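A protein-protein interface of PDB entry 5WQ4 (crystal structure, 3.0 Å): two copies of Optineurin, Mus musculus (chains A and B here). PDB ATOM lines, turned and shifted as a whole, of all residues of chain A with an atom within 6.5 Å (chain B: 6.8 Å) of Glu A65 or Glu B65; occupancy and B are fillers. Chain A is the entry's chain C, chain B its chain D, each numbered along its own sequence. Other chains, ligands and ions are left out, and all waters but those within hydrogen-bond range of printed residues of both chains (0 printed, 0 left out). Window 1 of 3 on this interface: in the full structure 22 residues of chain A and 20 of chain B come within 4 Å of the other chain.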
ATOM      1  N   SER A  60      -5.279  23.810 -24.555  1.00  0.00           N
ATOM      2  CA  SER A  60      -4.859  22.422 -24.307  1.00  0.00           C
ATOM      3  C   SER A  60      -3.338  22.302 -24.203  1.00  0.00           C
ATOM      4  O   SER A  60      -2.783  21.670 -23.297  1.00  0.00           O
ATOM      5  CB  SER A  60      -5.357  21.514 -25.446  1.00  0.00           C
ATOM      6  OG  SER A  60      -5.939  20.312 -24.967  1.00  0.00           O
ATOM      7  N   ASP A  61      -2.688  22.951 -25.156  1.00  0.00           N
ATOM      8  CA  ASP A  61      -1.254  22.918 -25.308  1.00  0.00           C
ATOM      9  C   ASP A  61      -0.615  23.532 -24.118  1.00  0.00           C
ATOM     10  O   ASP A  61       0.372  23.000 -23.596  1.00  0.00           O
ATOM     11  CB  ASP A  61      -0.832  23.677 -26.566  1.00  0.00           C
ATOM     12  CG  ASP A  61      -1.387  23.068 -27.819  1.00  0.00           C
ATOM     13  OD1 ASP A  61      -1.601  21.836 -27.844  1.00  0.00           O
ATOM     14  OD2 ASP A  61      -1.616  23.829 -28.776  1.00  0.00           O
ATOM     15  N   PHE A  62      -1.179  24.667 -23.704  1.00  0.00           N
ATOM     16  CA  PHE A  62      -0.727  25.358 -22.501  1.00  0.00           C
ATOM     17  C   PHE A  62      -0.809  24.494 -21.217  1.00  0.00           C
ATOM     18  O   PHE A  62       0.149  24.437 -20.438  1.00  0.00           O
ATOM     19  CB  PHE A  62      -1.555  26.601 -22.285  1.00  0.00           C
ATOM     20  CG  PHE A  62      -1.479  27.121 -20.883  1.00  0.00           C
ATOM     21  CD1 PHE A  62      -0.316  27.739 -20.422  1.00  0.00           C
ATOM     22  CD2 PHE A  62      -2.522  26.909 -19.986  1.00  0.00           C
ATOM     23  CE1 PHE A  62      -0.239  28.200 -19.132  1.00  0.00           C
ATOM     24  CE2 PHE A  62      -2.424  27.343 -18.695  1.00  0.00           C
ATOM     25  CZ  PHE A  62      -1.290  27.988 -18.269  1.00  0.00           C
ATOM     26  N   HIS A  63      -1.942  23.827 -20.991  1.00  0.00           N
ATOM     27  CA  HIS A  63      -2.047  22.962 -19.810  1.00  0.00           C
ATOM     28  C   HIS A  63      -1.068  21.789 -19.867  1.00  0.00           C
ATOM     29  O   HIS A  63      -0.453  21.428 -18.870  1.00  0.00           O
ATOM     30  CB  HIS A  63      -3.474  22.427 -19.646  1.00  0.00           C
ATOM     31  CG  HIS A  63      -4.462  23.463 -19.215  1.00  0.00           C
ATOM     32  ND1 HIS A  63      -4.364  24.127 -18.011  1.00  0.00           N
ATOM     33  CD2 HIS A  63      -5.549  23.975 -19.840  1.00  0.00           C
ATOM     34  CE1 HIS A  63      -5.359  24.989 -17.905  1.00  0.00           C
ATOM     35  NE2 HIS A  63      -6.091  24.922 -19.003  1.00  0.00           N
ATOM     36  N   ALA A  64      -0.915  21.214 -21.052  1.00  0.00           N
ATOM     37  CA  ALA A  64       0.020  20.119 -21.297  1.00  0.00           C
ATOM     38  C   ALA A  64       1.427  20.517 -20.932  1.00  0.00           C
ATOM     39  O   ALA A  64       2.193  19.758 -20.348  1.00  0.00           O
ATOM     40  CB  ALA A  64      -0.048  19.714 -22.746  1.00  0.00           C
ATOM     41  N   GLU A  65       1.768  21.724 -21.336  1.00  0.00           N
ATOM     42  CA  GLU A  65       3.084  22.277 -21.115  1.00  0.00           C
ATOM     43  C   GLU A  65       3.332  22.684 -19.672  1.00  0.00           C
ATOM     44  O   GLU A  65       4.426  22.520 -19.154  1.00  0.00           O
ATOM     45  CB  GLU A  65       3.267  23.483 -22.038  1.00  0.00           C
ATOM     46  CG  GLU A  65       4.563  23.489 -22.762  1.00  0.00           C
ATOM     47  CD  GLU A  65       4.512  22.686 -23.998  1.00  0.00           C
ATOM     48  OE1 GLU A  65       3.414  22.501 -24.537  1.00  0.00           O
ATOM     49  OE2 GLU A  65       5.570  22.229 -24.433  1.00  0.00           O
ATOM     50  N   ARG A  66       2.312  23.211 -19.013  1.00  0.00           N
ATOM     51  CA  ARG A  66       2.465  23.516 -17.615  1.00  0.00           C
ATOM     52  C   ARG A  66       2.664  22.274 -16.828  1.00  0.00           C
ATOM     53  O   ARG A  66       3.453  22.279 -15.875  1.00  0.00           O
ATOM     54  CB  ARG A  66       1.276  24.259 -17.044  1.00  0.00           C
ATOM     55  CG  ARG A  66       1.600  24.660 -15.643  1.00  0.00           C
ATOM     56  CD  ARG A  66       0.484  25.356 -14.968  1.00  0.00           C
ATOM     57  NE  ARG A  66       0.511  26.822 -14.962  1.00  0.00           N
ATOM     58  CZ  ARG A  66       1.558  27.637 -15.084  1.00  0.00           C
ATOM     59  NH1 ARG A  66       2.801  27.197 -15.254  1.00  0.00           N
ATOM     60  NH2 ARG A  66       1.332  28.945 -15.035  1.00  0.00           N
ATOM     61  N   ALA A  67       1.958  21.216 -17.223  1.00  0.00           N
ATOM     62  CA  ALA A  67       2.102  19.937 -16.555  1.00  0.00           C
ATOM     63  C   ALA A  67       3.537  19.433 -16.699  1.00  0.00           C
ATOM     64  O   ALA A  67       4.183  19.078 -15.709  1.00  0.00           O
ATOM     65  CB  ALA A  67       1.131  18.944 -17.095  1.00  0.00           C
ATOM     66  N   ALA A  68       4.050  19.443 -17.923  1.00  0.00           N
ATOM     67  CA  ALA A  68       5.437  19.059 -18.175  1.00  0.00           C
ATOM     68  C   ALA A  68       6.466  19.865 -17.355  1.00  0.00           C
ATOM     69  O   ALA A  68       7.422  19.328 -16.817  1.00  0.00           O
ATOM     70  CB  ALA A  68       5.715  19.201 -19.634  1.00  0.00           C
ATOM     71  N   ARG A  69       6.256  21.163 -17.287  1.00  0.00           N
ATOM     72  CA  ARG A  69       7.095  22.065 -16.543  1.00  0.00           C
ATOM     73  C   ARG A  69       7.101  21.693 -15.059  1.00  0.00           C
ATOM     74  O   ARG A  69       8.127  21.712 -14.385  1.00  0.00           O
ATOM     75  CB  ARG A  69       6.570  23.477 -16.786  1.00  0.00           C
ATOM     76  CG  ARG A  69       7.498  24.618 -16.457  1.00  0.00           C
ATOM     77  CD  ARG A  69       6.681  25.830 -16.067  1.00  0.00           C
ATOM     78  NE  ARG A  69       7.537  26.991 -15.870  1.00  0.00           N
ATOM     79  CZ  ARG A  69       7.098  28.246 -15.795  1.00  0.00           C
ATOM     80  NH1 ARG A  69       5.803  28.535 -15.931  1.00  0.00           N
ATOM     81  NH2 ARG A  69       7.968  29.220 -15.605  1.00  0.00           N
ATOM     82  N   GLU A  70       5.917  21.386 -14.544  1.00  0.00           N
ATOM     83  CA  GLU A  70       5.759  20.996 -13.147  1.00  0.00           C
ATOM     84  C   GLU A  70       6.459  19.692 -12.802  1.00  0.00           C
ATOM     85  O   GLU A  70       7.106  19.570 -11.753  1.00  0.00           O
ATOM     86  CB  GLU A  70       4.284  20.898 -12.830  1.00  0.00           C
ATOM     87  CG  GLU A  70       3.765  22.164 -12.270  1.00  0.00           C
ATOM     88  CD  GLU A  70       2.274  22.304 -12.339  1.00  0.00           C
ATOM     89  OE1 GLU A  70       1.738  23.238 -11.693  1.00  0.00           O
ATOM     90  OE2 GLU A  70       1.625  21.443 -12.956  1.00  0.00           O
ATOM     91  N   SER B  60      -0.070  32.982 -27.517  1.00  0.00           N
ATOM     92  CA  SER B  60       1.045  33.691 -26.897  1.00  0.00           C
ATOM     93  C   SER B  60       1.474  33.019 -25.568  1.00  0.00           C
ATOM     94  O   SER B  60       2.666  32.784 -25.318  1.00  0.00           O
ATOM     95  CB  SER B  60       0.652  35.163 -26.674  1.00  0.00           C
ATOM     96  OG  SER B  60       1.763  36.042 -26.764  1.00  0.00           O
ATOM     97  N   ASP B  61       0.480  32.705 -24.738  1.00  0.00           N
ATOM     98  CA  ASP B  61       0.687  32.076 -23.441  1.00  0.00           C
ATOM     99  C   ASP B  61       1.247  30.675 -23.569  1.00  0.00           C
ATOM    100  O   ASP B  61       2.211  30.304 -22.892  1.00  0.00           O
ATOM    101  CB  ASP B  61      -0.631  32.033 -22.669  1.00  0.00           C
ATOM    102  CG  ASP B  61      -1.116  33.413 -22.262  1.00  0.00           C
ATOM    103  OD1 ASP B  61      -0.278  34.276 -21.918  1.00  0.00           O
ATOM    104  OD2 ASP B  61      -2.335  33.647 -22.358  1.00  0.00           O
ATOM    105  N   PHE B  62       0.663  29.908 -24.467  1.00  0.00           N
ATOM    106  CA  PHE B  62       1.183  28.594 -24.735  1.00  0.00           C
ATOM    107  C   PHE B  62       2.642  28.608 -25.155  1.00  0.00           C
ATOM    108  O   PHE B  62       3.421  27.772 -24.694  1.00  0.00           O
ATOM    109  CB  PHE B  62       0.316  27.898 -25.775  1.00  0.00           C
ATOM    110  CG  PHE B  62       1.051  26.896 -26.588  1.00  0.00           C
ATOM    111  CD1 PHE B  62       1.681  25.819 -25.997  1.00  0.00           C
ATOM    112  CD2 PHE B  62       1.036  26.979 -27.966  1.00  0.00           C
ATOM    113  CE1 PHE B  62       2.361  24.913 -26.759  1.00  0.00           C
ATOM    114  CE2 PHE B  62       1.686  26.052 -28.722  1.00  0.00           C
ATOM    115  CZ  PHE B  62       2.348  25.020 -28.118  1.00  0.00           C
ATOM    116  N   HIS B  63       3.013  29.533 -26.030  1.00  0.00           N
ATOM    117  CA  HIS B  63       4.411  29.639 -26.436  1.00  0.00           C
ATOM    118  C   HIS B  63       5.316  30.045 -25.253  1.00  0.00           C
ATOM    119  O   HIS B  63       6.447  29.570 -25.122  1.00  0.00           O
ATOM    120  CB  HIS B  63       4.549  30.623 -27.603  1.00  0.00           C
ATOM    121  CG  HIS B  63       3.992  30.116 -28.902  1.00  0.00           C
ATOM    122  ND1 HIS B  63       4.447  28.965 -29.512  1.00  0.00           N
ATOM    123  CD2 HIS B  63       3.057  30.633 -29.735  1.00  0.00           C
ATOM    124  CE1 HIS B  63       3.794  28.777 -30.645  1.00  0.00           C
ATOM    125  NE2 HIS B  63       2.945  29.775 -30.806  1.00  0.00           N
ATOM    126  N   ALA B  64       4.826  30.939 -24.403  1.00  0.00           N
ATOM    127  CA  ALA B  64       5.573  31.306 -23.211  1.00  0.00           C
ATOM    128  C   ALA B  64       5.841  30.085 -22.319  1.00  0.00           C
ATOM    129  O   ALA B  64       6.977  29.866 -21.854  1.00  0.00           O
ATOM    130  CB  ALA B  64       4.829  32.377 -22.437  1.00  0.00           C
ATOM    131  N   GLU B  65       4.804  29.269 -22.104  1.00  0.00           N
ATOM    132  CA  GLU B  65       4.922  28.113 -21.222  1.00  0.00           C
ATOM    133  C   GLU B  65       5.794  27.039 -21.816  1.00  0.00           C
ATOM    134  O   GLU B  65       6.450  26.316 -21.069  1.00  0.00           O
ATOM    135  CB  GLU B  65       3.562  27.518 -20.896  1.00  0.00           C
ATOM    136  CG  GLU B  65       2.979  28.045 -19.596  1.00  0.00           C
ATOM    137  CD  GLU B  65       3.555  27.398 -18.378  1.00  0.00           C
ATOM    138  OE1 GLU B  65       3.826  26.193 -18.451  1.00  0.00           O
ATOM    139  OE2 GLU B  65       3.725  28.087 -17.348  1.00  0.00           O
ATOM    140  N   ARG B  66       5.764  26.902 -23.140  1.00  0.00           N
ATOM    141  CA  ARG B  66       6.674  26.008 -23.829  1.00  0.00           C
ATOM    142  C   ARG B  66       8.088  26.468 -23.698  1.00  0.00           C
ATOM    143  O   ARG B  66       8.992  25.647 -23.631  1.00  0.00           O
ATOM    144  CB  ARG B  66       6.290  25.881 -25.276  1.00  0.00           C
ATOM    145  CG  ARG B  66       6.769  24.621 -25.980  1.00  0.00           C
ATOM    146  CD  ARG B  66       7.392  24.978 -27.308  1.00  0.00           C
ATOM    147  NE  ARG B  66       6.396  25.571 -28.201  1.00  0.00           N
ATOM    148  CZ  ARG B  66       6.345  25.375 -29.514  1.00  0.00           C
ATOM    149  NH1 ARG B  66       7.256  24.619 -30.102  1.00  0.00           N
ATOM    150  NH2 ARG B  66       5.396  25.949 -30.246  1.00  0.00           N
ATOM    151  N   ALA B  67       8.296  27.784 -23.697  1.00  0.00           N
ATOM    152  CA  ALA B  67       9.648  28.343 -23.544  1.00  0.00           C
ATOM    153  C   ALA B  67      10.185  27.980 -22.187  1.00  0.00           C
ATOM    154  O   ALA B  67      11.278  27.435 -22.076  1.00  0.00           O
ATOM    155  CB  ALA B  67       9.642  29.845 -23.721  1.00  0.00           C
ATOM    156  N   ALA B  68       9.373  28.273 -21.166  1.00  0.00           N
ATOM    157  CA  ALA B  68       9.658  27.935 -19.767  1.00  0.00           C
ATOM    158  C   ALA B  68       9.904  26.457 -19.540  1.00  0.00           C
ATOM    159  O   ALA B  68      10.804  26.074 -18.802  1.00  0.00           O
ATOM    160  CB  ALA B  68       8.513  28.387 -18.890  1.00  0.00           C
ATOM    161  N   ARG B  69       9.061  25.640 -20.156  1.00  0.00           N
ATOM    162  CA  ARG B  69       9.171  24.210 -20.101  1.00  0.00           C
ATOM    163  C   ARG B  69      10.486  23.750 -20.678  1.00  0.00           C
ATOM    164  O   ARG B  69      11.179  22.892 -20.119  1.00  0.00           O
ATOM    165  CB  ARG B  69       8.054  23.565 -20.879  1.00  0.00           C
ATOM    166  CG  ARG B  69       7.873  22.126 -20.524  1.00  0.00           C
ATOM    167  CD  ARG B  69       7.554  21.345 -21.750  1.00  0.00           C
ATOM    168  NE  ARG B  69       8.805  20.892 -22.330  1.00  0.00           N
ATOM    169  CZ  ARG B  69       9.090  20.905 -23.622  1.00  0.00           C
ATOM    170  NH1 ARG B  69      10.271  20.461 -24.027  1.00  0.00           N
ATOM    171  NH2 ARG B  69       8.207  21.356 -24.502  1.00  0.00           N
ATOM    172  N   GLU B  70      10.824  24.327 -21.822  1.00  0.00           N
ATOM    173  CA  GLU B  70      12.038  23.972 -22.539  1.00  0.00           C
ATOM    174  C   GLU B  70      13.287  24.360 -21.733  1.00  0.00           C
ATOM    175  O   GLU B  70      14.244  23.596 -21.644  1.00  0.00           O
ATOM    176  CB  GLU B  70      12.007  24.627 -23.923  1.00  0.00           C
ATOM    177  CG  GLU B  70      11.321  23.760 -24.995  1.00  0.00           C
ATOM    178  CD  GLU B  70      10.851  24.526 -26.252  1.00  0.00           C
ATOM    179  OE1 GLU B  70      11.005  25.764 -26.342  1.00  0.00           O
ATOM    180  OE2 GLU B  70      10.294  23.870 -27.160  1.00  0.00           O
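NH2 of Arg B69 lies within salt-bridge range of OE2 of Glu A65, at 2.8 Å. NH1 of Arg A66 lies within salt-bridge range of OE2 of Glu B65, at 2.5 Å. OE2 of Glu B65 is in salt-bridge range of NH1 of Arg A69.
ND1 of His B63 lies within hydrogen-bond range of NH2 of Arg B66 (3.2 Å).
Phe B62 touches Asp A61. Phe B62 touches Phe A62 (CD1 to N, 3.8 Å). CG of Glu B65 touches CE1 of Phe A62, at 3.3 Å. Glu A65 touches Phe B62. Glu A65 touches Glu B65 (C to OE1, 3.7 Å). CG of Arg B66 touches OE2 of Glu A65 (3.1 Å). CB of Ala A68 touches CD of Arg B69, 3.5 Å away. CZ of Arg A69 touches CB of Ala B68, 3.4 Å away. Arg A69 touches Arg B69.
Of the printed residues of chain B, Asp A61 touches Phe B62 (3.4 Å). Of chain B, only Phe B62 (3.4 Å), Glu B65 (3.7 Å), Arg B66 (3.1 Å) and Arg B69 (2.8 Å) come within 4 Å of Glu A65. Ala A67 touches none of the printed residues of chain B. Printed residues of chain B within 4 Å of Ala A68: Arg B69. Glu B65 touches just these residues of chain A: Phe A62 (3.3 Å), Glu A65 (3.7 Å), Arg A66 (2.5 Å) and Arg A69 (2.6 Å). The nearest residue of chain B that does not touch Glu A65 is Glu B70 (5.7 Å).
Of the 11 printed residues of chain B, 5 touch a printed residue of chain A. Hydrophobic or aromatic side chains of chain B within 4 Å of the printed part of chain A: Phe B62 and Ala B68. Of the 11 printed residues of chain A, 6 touch a printed residue of chain B. Along chain A the printed residues that touch a printed residue of chain B span positions 61 to 69. Among the printed residues, 12 pairs touch across the chains.
Asp A61 touches Phe B62, but with the chains exchanged Phe A62 does not touch Asp B61 (4.4 Å). Glu A65 touches Arg B66, and with the chains exchanged Arg A66 touches Glu B65. Ala A68 touches Arg B69, and with the chains exchanged Arg A69 touches Ala B68. Arg A69 touches its own counterpart, Arg B69.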
